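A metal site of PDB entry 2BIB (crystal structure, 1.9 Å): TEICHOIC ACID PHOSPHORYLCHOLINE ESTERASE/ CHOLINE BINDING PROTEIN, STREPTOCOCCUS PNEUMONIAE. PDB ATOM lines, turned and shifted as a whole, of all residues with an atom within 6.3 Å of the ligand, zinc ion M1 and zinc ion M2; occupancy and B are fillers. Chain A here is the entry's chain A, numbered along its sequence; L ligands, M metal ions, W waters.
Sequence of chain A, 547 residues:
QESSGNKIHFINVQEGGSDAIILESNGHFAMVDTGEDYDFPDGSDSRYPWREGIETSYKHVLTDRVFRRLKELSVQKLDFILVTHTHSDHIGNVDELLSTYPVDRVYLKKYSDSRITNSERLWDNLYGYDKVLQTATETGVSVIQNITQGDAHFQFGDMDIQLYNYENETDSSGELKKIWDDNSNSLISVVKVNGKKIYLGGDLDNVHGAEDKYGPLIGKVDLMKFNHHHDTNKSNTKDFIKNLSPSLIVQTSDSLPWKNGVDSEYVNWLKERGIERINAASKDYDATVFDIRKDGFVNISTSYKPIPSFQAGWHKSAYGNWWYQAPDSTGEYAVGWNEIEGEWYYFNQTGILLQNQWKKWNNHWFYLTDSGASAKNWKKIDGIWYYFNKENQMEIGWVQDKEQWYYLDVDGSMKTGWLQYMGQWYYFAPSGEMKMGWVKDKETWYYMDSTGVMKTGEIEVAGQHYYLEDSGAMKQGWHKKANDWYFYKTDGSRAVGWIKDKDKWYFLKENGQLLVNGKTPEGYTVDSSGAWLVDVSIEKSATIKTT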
ATOM      1  N   GLY A  17       7.722  -0.374  21.263  1.00  0.00           N
ATOM      2  CA  GLY A  17       8.530   0.394  22.181  1.00  0.00           C
ATOM      3  C   GLY A  17       8.323  -0.023  23.606  1.00  0.00           C
ATOM      4  O   GLY A  17       7.195  -0.265  24.041  1.00  0.00           O
ATOM      5  N   SER A  18       9.437  -0.094  24.346  1.00  0.00           N
ATOM      6  CA  SER A  18       9.432  -0.451  25.762  1.00  0.00           C
ATOM      7  C   SER A  18      10.794  -0.136  26.376  1.00  0.00           C
ATOM      8  O   SER A  18      11.814  -0.332  25.727  1.00  0.00           O
ATOM      9  CB  SER A  18       9.087  -1.947  25.947  1.00  0.00           C
ATOM     10  OG  SER A  18       9.078  -2.286  27.338  1.00  0.00           O
ATOM     11  N   ASP A  19      10.783   0.328  27.625  1.00  0.00           N
ATOM     12  CA  ASP A  19      11.997   0.749  28.339  1.00  0.00           C
ATOM     13  C   ASP A  19      12.351  -0.224  29.449  1.00  0.00           C
ATOM     14  O   ASP A  19      11.589  -0.391  30.387  1.00  0.00           O
ATOM     15  CB  ASP A  19      11.792   2.101  29.015  1.00  0.00           C
ATOM     16  CG  ASP A  19      11.816   3.279  28.059  1.00  0.00           C
ATOM     17  OD1 ASP A  19      11.492   3.112  26.874  1.00  0.00           O
ATOM     18  OD2 ASP A  19      12.125   4.444  28.446  1.00  0.00           O
ATOM     19  N   GLU A  36       8.038  -4.257  29.435  1.00  0.00           N
ATOM     20  CA  GLU A  36       6.747  -4.941  29.421  1.00  0.00           C
ATOM     21  C   GLU A  36       6.847  -6.352  29.976  1.00  0.00           C
ATOM     22  O   GLU A  36       7.832  -7.072  29.712  1.00  0.00           O
ATOM     23  CB  GLU A  36       6.186  -4.997  27.973  1.00  0.00           C
ATOM     24  CG  GLU A  36       4.760  -5.536  27.864  1.00  0.00           C
ATOM     25  CD  GLU A  36       3.755  -4.637  28.584  1.00  0.00           C
ATOM     26  OE1 GLU A  36       3.539  -3.506  28.101  1.00  0.00           O
ATOM     27  OE2 GLU A  36       3.194  -5.071  29.639  1.00  0.00           O
ATOM     28  N   GLY A  53      -6.642  -1.702  24.457  1.00  0.00           N
ATOM     29  CA  GLY A  53      -5.261  -1.272  24.373  1.00  0.00           C
ATOM     30  C   GLY A  53      -4.303  -1.873  25.406  1.00  0.00           C
ATOM     31  O   GLY A  53      -3.090  -1.704  25.272  1.00  0.00           O
ATOM     32  N   ILE A  54      -4.816  -2.549  26.430  1.00  0.00           N
ATOM     33  CA  ILE A  54      -3.927  -3.225  27.393  1.00  0.00           C
ATOM     34  C   ILE A  54      -3.062  -4.244  26.628  1.00  0.00           C
ATOM     35  O   ILE A  54      -3.605  -5.057  25.857  1.00  0.00           O
ATOM     36  CB  ILE A  54      -4.720  -3.939  28.516  1.00  0.00           C
ATOM     37  CG1 ILE A  54      -5.375  -2.925  29.476  1.00  0.00           C
ATOM     38  CG2 ILE A  54      -3.826  -4.932  29.285  1.00  0.00           C
ATOM     39  CD1 ILE A  54      -6.354  -3.568  30.461  1.00  0.00           C
ATOM     40  N   GLU A  55      -1.748  -4.203  26.837  1.00  0.00           N
ATOM     41  CA  GLU A  55      -0.799  -5.121  26.147  1.00  0.00           C
ATOM     42  C   GLU A  55      -0.999  -6.619  26.479  1.00  0.00           C
ATOM     43  O   GLU A  55      -1.019  -6.995  27.657  1.00  0.00           O
ATOM     44  CB  GLU A  55       0.655  -4.722  26.453  1.00  0.00           C
ATOM     45  CG  GLU A  55       1.704  -5.468  25.640  1.00  0.00           C
ATOM     46  CD  GLU A  55       1.558  -5.184  24.163  1.00  0.00           C
ATOM     47  OE1 GLU A  55       1.996  -4.100  23.722  1.00  0.00           O
ATOM     48  OE2 GLU A  55       0.971  -6.007  23.465  1.00  0.00           O
ATOM     49  N   HIS A  85       7.152   5.925  35.130  1.00  0.00           N
ATOM     50  CA  HIS A  85       5.701   6.097  35.168  1.00  0.00           C
ATOM     51  C   HIS A  85       4.999   4.732  35.179  1.00  0.00           C
ATOM     52  O   HIS A  85       5.666   3.708  35.136  1.00  0.00           O
ATOM     53  CB  HIS A  85       5.199   7.031  34.028  1.00  0.00           C
ATOM     54  CG  HIS A  85       5.392   6.508  32.632  1.00  0.00           C
ATOM     55  ND1 HIS A  85       6.633   6.172  32.123  1.00  0.00           N
ATOM     56  CD2 HIS A  85       4.499   6.326  31.623  1.00  0.00           C
ATOM     57  CE1 HIS A  85       6.484   5.793  30.863  1.00  0.00           C
ATOM     58  NE2 HIS A  85       5.202   5.872  30.532  1.00  0.00           N
ATOM     59  N   THR A  86       3.665   4.710  35.194  1.00  0.00           N
ATOM     60  CA  THR A  86       2.925   3.449  35.440  1.00  0.00           C
ATOM     61  C   THR A  86       2.553   2.624  34.195  1.00  0.00           C
ATOM     62  O   THR A  86       1.903   1.581  34.303  1.00  0.00           O
ATOM     63  CB  THR A  86       1.649   3.743  36.256  1.00  0.00           C
ATOM     64  OG1 THR A  86       0.825   4.679  35.538  1.00  0.00           O
ATOM     65  CG2 THR A  86       1.990   4.458  37.583  1.00  0.00           C
ATOM     66  N   HIS A  87       2.960   3.084  33.025  1.00  0.00           N
ATOM     67  CA  HIS A  87       2.675   2.332  31.803  1.00  0.00           C
ATOM     68  C   HIS A  87       3.341   0.955  31.824  1.00  0.00           C
ATOM     69  O   HIS A  87       4.497   0.821  32.212  1.00  0.00           O
ATOM     70  CB  HIS A  87       3.037   3.158  30.550  1.00  0.00           C
ATOM     71  CG  HIS A  87       2.107   4.328  30.337  1.00  0.00           C
ATOM     72  ND1 HIS A  87       2.413   5.391  29.503  1.00  0.00           N
ATOM     73  CD2 HIS A  87       0.890   4.609  30.878  1.00  0.00           C
ATOM     74  CE1 HIS A  87       1.415   6.268  29.539  1.00  0.00           C
ATOM     75  NE2 HIS A  87       0.482   5.807  30.354  1.00  0.00           N
ATOM     76  N   SER A  88       2.579  -0.064  31.440  1.00  0.00           N
ATOM     77  CA  SER A  88       2.998  -1.452  31.517  1.00  0.00           C
ATOM     78  C   SER A  88       4.366  -1.701  30.864  1.00  0.00           C
ATOM     79  O   SER A  88       5.105  -2.576  31.288  1.00  0.00           O
ATOM     80  CB  SER A  88       1.939  -2.351  30.877  1.00  0.00           C
ATOM     81  OG  SER A  88       1.881  -2.133  29.477  1.00  0.00           O
ATOM     82  N   ASP A  89       4.697  -0.935  29.826  1.00  0.00           N
ATOM     83  CA  ASP A  89       5.938  -1.146  29.076  1.00  0.00           C
ATOM     84  C   ASP A  89       7.168  -0.546  29.777  1.00  0.00           C
ATOM     85  O   ASP A  89       8.288  -0.614  29.250  1.00  0.00           O
ATOM     86  CB  ASP A  89       5.834  -0.644  27.623  1.00  0.00           C
ATOM     87  CG  ASP A  89       5.535   0.843  27.526  1.00  0.00           C
ATOM     88  OD1 ASP A  89       4.527   1.270  28.125  1.00  0.00           O
ATOM     89  OD2 ASP A  89       6.243   1.666  26.887  1.00  0.00           O
ATOM     90  N   HIS A  90       6.934   0.016  30.970  1.00  0.00           N
ATOM     91  CA  HIS A  90       7.967   0.587  31.839  1.00  0.00           C
ATOM     92  C   HIS A  90       7.976  -0.108  33.213  1.00  0.00           C
ATOM     93  O   HIS A  90       9.025  -0.594  33.659  1.00  0.00           O
ATOM     94  CB  HIS A  90       7.745   2.093  31.975  1.00  0.00           C
ATOM     95  CG  HIS A  90       7.837   2.807  30.657  1.00  0.00           C
ATOM     96  ND1 HIS A  90       8.956   3.511  30.269  1.00  0.00           N
ATOM     97  CD2 HIS A  90       6.959   2.911  29.625  1.00  0.00           C
ATOM     98  CE1 HIS A  90       8.756   4.028  29.069  1.00  0.00           C
ATOM     99  NE2 HIS A  90       7.558   3.674  28.650  1.00  0.00           N
ATOM    100  N   ARG A 121      -6.930   6.433  28.526  1.00  0.00           N
ATOM    101  CA  ARG A 121      -5.486   6.323  28.777  1.00  0.00           C
ATOM    102  C   ARG A 121      -5.220   5.769  30.196  1.00  0.00           C
ATOM    103  O   ARG A 121      -4.250   6.150  30.872  1.00  0.00           O
ATOM    104  CB  ARG A 121      -4.802   7.696  28.547  1.00  0.00           C
ATOM    105  CG  ARG A 121      -5.059   8.295  27.107  1.00  0.00           C
ATOM    106  CD  ARG A 121      -4.134   9.472  26.694  1.00  0.00           C
ATOM    107  NE  ARG A 121      -2.859   8.971  26.148  1.00  0.00           N
ATOM    108  CZ  ARG A 121      -2.630   8.687  24.859  1.00  0.00           C
ATOM    109  NH1 ARG A 121      -3.563   8.879  23.930  1.00  0.00           N
ATOM    110  NH2 ARG A 121      -1.447   8.207  24.502  1.00  0.00           N
ATOM    111  N   TRP A 123      -5.820   2.152  30.807  1.00  0.00           N
ATOM    112  CA  TRP A 123      -5.313   0.806  30.500  1.00  0.00           C
ATOM    113  C   TRP A 123      -5.191  -0.054  31.786  1.00  0.00           C
ATOM    114  O   TRP A 123      -6.158  -0.210  32.541  1.00  0.00           O
ATOM    115  CB  TRP A 123      -3.963   0.923  29.748  1.00  0.00           C
ATOM    116  CG  TRP A 123      -4.082   1.659  28.413  1.00  0.00           C
ATOM    117  CD1 TRP A 123      -4.826   1.287  27.342  1.00  0.00           C
ATOM    118  CD2 TRP A 123      -3.431   2.896  28.042  1.00  0.00           C
ATOM    119  NE1 TRP A 123      -4.682   2.198  26.319  1.00  0.00           N
ATOM    120  CE2 TRP A 123      -3.835   3.198  26.719  1.00  0.00           C
ATOM    121  CE3 TRP A 123      -2.548   3.771  28.696  1.00  0.00           C
ATOM    122  CZ2 TRP A 123      -3.384   4.343  26.036  1.00  0.00           C
ATOM    123  CZ3 TRP A 123      -2.100   4.906  28.010  1.00  0.00           C
ATOM    124  CH2 TRP A 123      -2.524   5.189  26.697  1.00  0.00           C
ATOM    125  N   ASP A 124      -3.990  -0.594  32.007  1.00  0.00           N
ATOM    126  CA  ASP A 124      -3.665  -1.301  33.247  1.00  0.00           C
ATOM    127  C   ASP A 124      -2.584  -0.581  34.075  1.00  0.00           C
ATOM    128  O   ASP A 124      -1.742  -1.225  34.705  1.00  0.00           O
ATOM    129  CB  ASP A 124      -3.197  -2.726  32.948  1.00  0.00           C
ATOM    130  CG  ASP A 124      -2.004  -2.781  31.999  1.00  0.00           C
ATOM    131  OD1 ASP A 124      -1.671  -1.775  31.324  1.00  0.00           O
ATOM    132  OD2 ASP A 124      -1.321  -3.816  31.905  1.00  0.00           O
ATOM    133  N   ASN A 125      -2.626   0.762  34.064  1.00  0.00           N
ATOM    134  CA  ASN A 125      -1.686   1.575  34.836  1.00  0.00           C
ATOM    135  C   ASN A 125      -1.771   1.221  36.336  1.00  0.00           C
ATOM    136  O   ASN A 125      -0.769   0.991  37.000  1.00  0.00           O
ATOM    137  CB  ASN A 125      -1.981   3.078  34.710  1.00  0.00           C
ATOM    138  CG  ASN A 125      -1.906   3.613  33.288  1.00  0.00           C
ATOM    139  OD1 ASN A 125      -1.396   2.959  32.376  1.00  0.00           O
ATOM    140  ND2 ASN A 125      -2.451   4.824  33.091  1.00  0.00           N
ATOM    141  N   ASP A 181      -2.095  12.121  30.484  1.00  0.00           N
ATOM    142  CA  ASP A 181      -1.500  10.812  30.296  1.00  0.00           C
ATOM    143  C   ASP A 181      -0.347  10.741  31.294  1.00  0.00           C
ATOM    144  O   ASP A 181       0.290  11.761  31.601  1.00  0.00           O
ATOM    145  CB  ASP A 181      -0.974  10.695  28.846  1.00  0.00           C
ATOM    146  CG  ASP A 181      -0.352   9.348  28.543  1.00  0.00           C
ATOM    147  OD1 ASP A 181      -1.055   8.413  28.074  1.00  0.00           O
ATOM    148  OD2 ASP A 181       0.847   9.141  28.738  1.00  0.00           O
ATOM    149  N   ASP A 182      -0.070   9.553  31.831  1.00  0.00           N
ATOM    150  CA  ASP A 182       1.011   9.436  32.811  1.00  0.00           C
ATOM    151  C   ASP A 182       2.410   9.739  32.276  1.00  0.00           C
ATOM    152  O   ASP A 182       3.337   9.977  33.047  1.00  0.00           O
ATOM    153  CB  ASP A 182       0.991   8.069  33.483  1.00  0.00           C
ATOM    154  CG  ASP A 182       1.456   8.136  34.915  1.00  0.00           C
ATOM    155  OD1 ASP A 182       2.046   7.142  35.414  1.00  0.00           O
ATOM    156  OD2 ASP A 182       1.282   9.162  35.612  1.00  0.00           O
ATOM    157  N   ASN A 183       2.576   9.739  30.948  1.00  0.00           N
ATOM    158  CA  ASN A 183       3.855  10.118  30.325  1.00  0.00           C
ATOM    159  C   ASN A 183       4.406  11.458  30.836  1.00  0.00           C
ATOM    160  O   ASN A 183       5.600  11.613  31.056  1.00  0.00           O
ATOM    161  CB  ASN A 183       3.716  10.193  28.805  1.00  0.00           C
ATOM    162  CG  ASN A 183       3.666   8.828  28.155  1.00  0.00           C
ATOM    163  OD1 ASN A 183       3.769   7.793  28.834  1.00  0.00           O
ATOM    164  ND2 ASN A 183       3.505   8.818  26.817  1.00  0.00           N
ATOM    165  N   SER A 186       6.627  11.511  33.953  1.00  0.00           N
ATOM    166  CA  SER A 186       7.876  10.747  33.912  1.00  0.00           C
ATOM    167  C   SER A 186       8.995  11.286  34.803  1.00  0.00           C
ATOM    168  O   SER A 186       9.390  12.458  34.700  1.00  0.00           O
ATOM    169  CB  SER A 186       8.411  10.594  32.470  1.00  0.00           C
ATOM    170  OG  SER A 186       7.537   9.800  31.700  1.00  0.00           O
ATOM    171  N   GLY A 202      12.270   8.485  30.478  1.00  0.00           N
ATOM    172  CA  GLY A 202      11.051   7.691  30.316  1.00  0.00           C
ATOM    173  C   GLY A 202      10.240   8.093  29.100  1.00  0.00           C
ATOM    174  O   GLY A 202      10.775   8.147  27.990  1.00  0.00           O
ATOM    175  N   ASP A 203       8.958   8.418  29.316  1.00  0.00           N
ATOM    176  CA  ASP A 203       8.038   8.767  28.217  1.00  0.00           C
ATOM    177  C   ASP A 203       7.700  10.261  28.281  1.00  0.00           C
ATOM    178  O   ASP A 203       6.650  10.689  27.818  1.00  0.00           O
ATOM    179  CB  ASP A 203       6.742   7.867  28.235  1.00  0.00           C
ATOM    180  CG  ASP A 203       6.965   6.458  27.645  1.00  0.00           C
ATOM    181  OD1 ASP A 203       6.049   5.510  27.696  1.00  0.00           O
ATOM    182  OD2 ASP A 203       8.084   6.214  27.107  1.00  0.00           O
ATOM    183  N   HIS A 228       9.676   8.853  25.080  1.00  0.00           N
ATOM    184  CA  HIS A 228       8.481   8.174  24.539  1.00  0.00           C
ATOM    185  C   HIS A 228       8.742   7.433  23.210  1.00  0.00           C
ATOM    186  O   HIS A 228       7.971   7.572  22.248  1.00  0.00           O
ATOM    187  CB  HIS A 228       7.306   9.166  24.417  1.00  0.00           C
ATOM    188  CG  HIS A 228       5.980   8.525  24.103  1.00  0.00           C
ATOM    189  ND1 HIS A 228       5.022   9.166  23.360  1.00  0.00           N
ATOM    190  CD2 HIS A 228       5.451   7.338  24.481  1.00  0.00           C
ATOM    191  CE1 HIS A 228       3.956   8.383  23.250  1.00  0.00           C
ATOM    192  NE2 HIS A 228       4.188   7.281  23.932  1.00  0.00           N
ATOM    193  N   HIS A 229       9.858   6.694  23.167  1.00  0.00           N
ATOM    194  CA  HIS A 229      10.151   5.679  22.143  1.00  0.00           C
ATOM    195  C   HIS A 229      10.448   6.212  20.732  1.00  0.00           C
ATOM    196  O   HIS A 229      11.526   5.927  20.180  1.00  0.00           O
ATOM    197  CB  HIS A 229       9.044   4.584  22.088  1.00  0.00           C
ATOM    198  CG  HIS A 229       8.716   4.009  23.441  1.00  0.00           C
ATOM    199  ND1 HIS A 229       9.569   3.151  24.121  1.00  0.00           N
ATOM    200  CD2 HIS A 229       7.639   4.178  24.235  1.00  0.00           C
ATOM    201  CE1 HIS A 229       9.014   2.818  25.270  1.00  0.00           C
ATOM    202  NE2 HIS A 229       7.847   3.425  25.371  1.00  0.00           N
HETATM  203  P1  LIG L   1       3.390   4.536  25.971  1.00  0.00           P
HETATM  204  O1  LIG L   1       3.055   4.861  24.434  1.00  0.00           O
HETATM  205  O2  LIG L   1       4.751   3.752  25.929  1.00  0.00           O
HETATM  206  O3  LIG L   1       3.366   5.825  26.841  1.00  0.00           O
HETATM  207  O4  LIG L   1       2.242   3.542  26.525  1.00  0.00           O
HETATM  208  C1  LIG L   1       1.431   2.908  25.541  1.00  0.00           C
HETATM  209  C2  LIG L   1       0.126   2.446  26.177  1.00  0.00           C
HETATM  210  N1  LIG L   1       0.226   1.131  26.847  1.00  0.00           N
HETATM  211  C3  LIG L   1      -0.935   0.338  26.435  1.00  0.00           C
HETATM  212  C4  LIG L   1       0.140   1.356  28.299  1.00  0.00           C
HETATM  213  C5  LIG L   1       1.478   0.383  26.542  1.00  0.00           C
HETATM  214 ZN    ZN M   1       4.255   5.887  28.641  1.00  0.00          ZN
HETATM  215 ZN    ZN M   2       6.465   3.650  26.890  1.00  0.00          ZN
HETATM  216  O   HOH W   1       5.205   1.597  24.091  1.00  0.00           O
HETATM  217  O   HOH W   2       0.678   7.226  26.211  1.00  0.00           O
HETATM  218  O   HOH W   3      -0.849  -2.274  28.752  1.00  0.00           O
HETATM  219  O   HOH W   4      -0.319   0.590  31.448  1.00  0.00           O
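Zinc ion M1 is bound by the side-chain amide oxygen (OD1) of Asn 183 (2.0 Å), an oxygen (O3) of the ligand (2.0 Å), the side-chain carboxylate (OD1) of Asp 203 (2.1 Å), a ring nitrogen (ND1) of His 87 (2.1 Å) and a ring nitrogen (NE2) of His 85 (2.1 Å). Zinc ion M1 has five donor atoms within binding distance.
Of the 25 residues printed, 5 come within 4 Å of zinc ion M1.
Zinc ion M2 is bound by O2 of the ligand. OD2 of Asp 89 binds zinc ion M2. NE2 of His 229 binds zinc ion M2. Zinc ion M2 is bound by the side-chain carboxylate (OD1) of Asp 203, 2.1 Å away. NE2 of His 90 is bound to zinc ion M2.
Merely in contact with the ligand: Gly 53 (3.2 Å), Trp 123 (3.6 Å) and Ser 88 (3.9 Å). Of the 25 residues printed, 10 come within 4 Å of the ligand.
A ring nitrogen (NE2) of His 228 is in hydrogen-bond range of an oxygen (O1) of the ligand (2.7 Å).
Water W2 lies within hydrogen-bond range of the side-chain carboxylate (OD1) of Asp 181 (2.8 Å), the guanidinium group (NH2) of Arg 121 (2.9 Å) and the side-chain amide nitrogen (ND2) of Asn 183 (3.3 Å). Water W4 lies within hydrogen-bond range of OD1 of Asp 124 (2.7 Å), OD1 of Asn 125 (2.8 Å) and N of Ser 88 (3.0 Å). Water W3 lies within hydrogen-bond range of the side-chain carboxylate of Asp 124 (2.7 Å), the side-chain hydroxyl of Ser 88 (2.8 Å) and the backbone NH of Glu 55 (2.9 Å).
The side-chain amide nitrogen (ND2) of Asn 183 lies within hydrogen-bond range of a ring nitrogen (NE2) of His 228 (3.3 Å). O of Asn 183 is in hydrogen-bond range of OG of Ser 186. The backbone NH of Asp 19 is in hydrogen-bond range of the backbone carbonyl oxygen of Asp 89 (3.1 Å). O of Asp 89 lies within hydrogen-bond range of OG of Ser 18, at 2.7 Å. OG of Ser 186 sits at hydrogen-bond distance from N of Asp 203, 3.1 Å away. A ring nitrogen (ND1) of His 229 lies close to the side-chain carboxylate of Asp 19 (3.4 Å). A ring nitrogen (ND1) of His 229 sits close to the backbone NH (N) of Ser 18 (3.3 Å). The side-chain hydroxyl (OG) of Ser 88 sits at hydrogen-bond distance from the side-chain carboxylate (OE1) of Glu 36 (2.6 Å).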
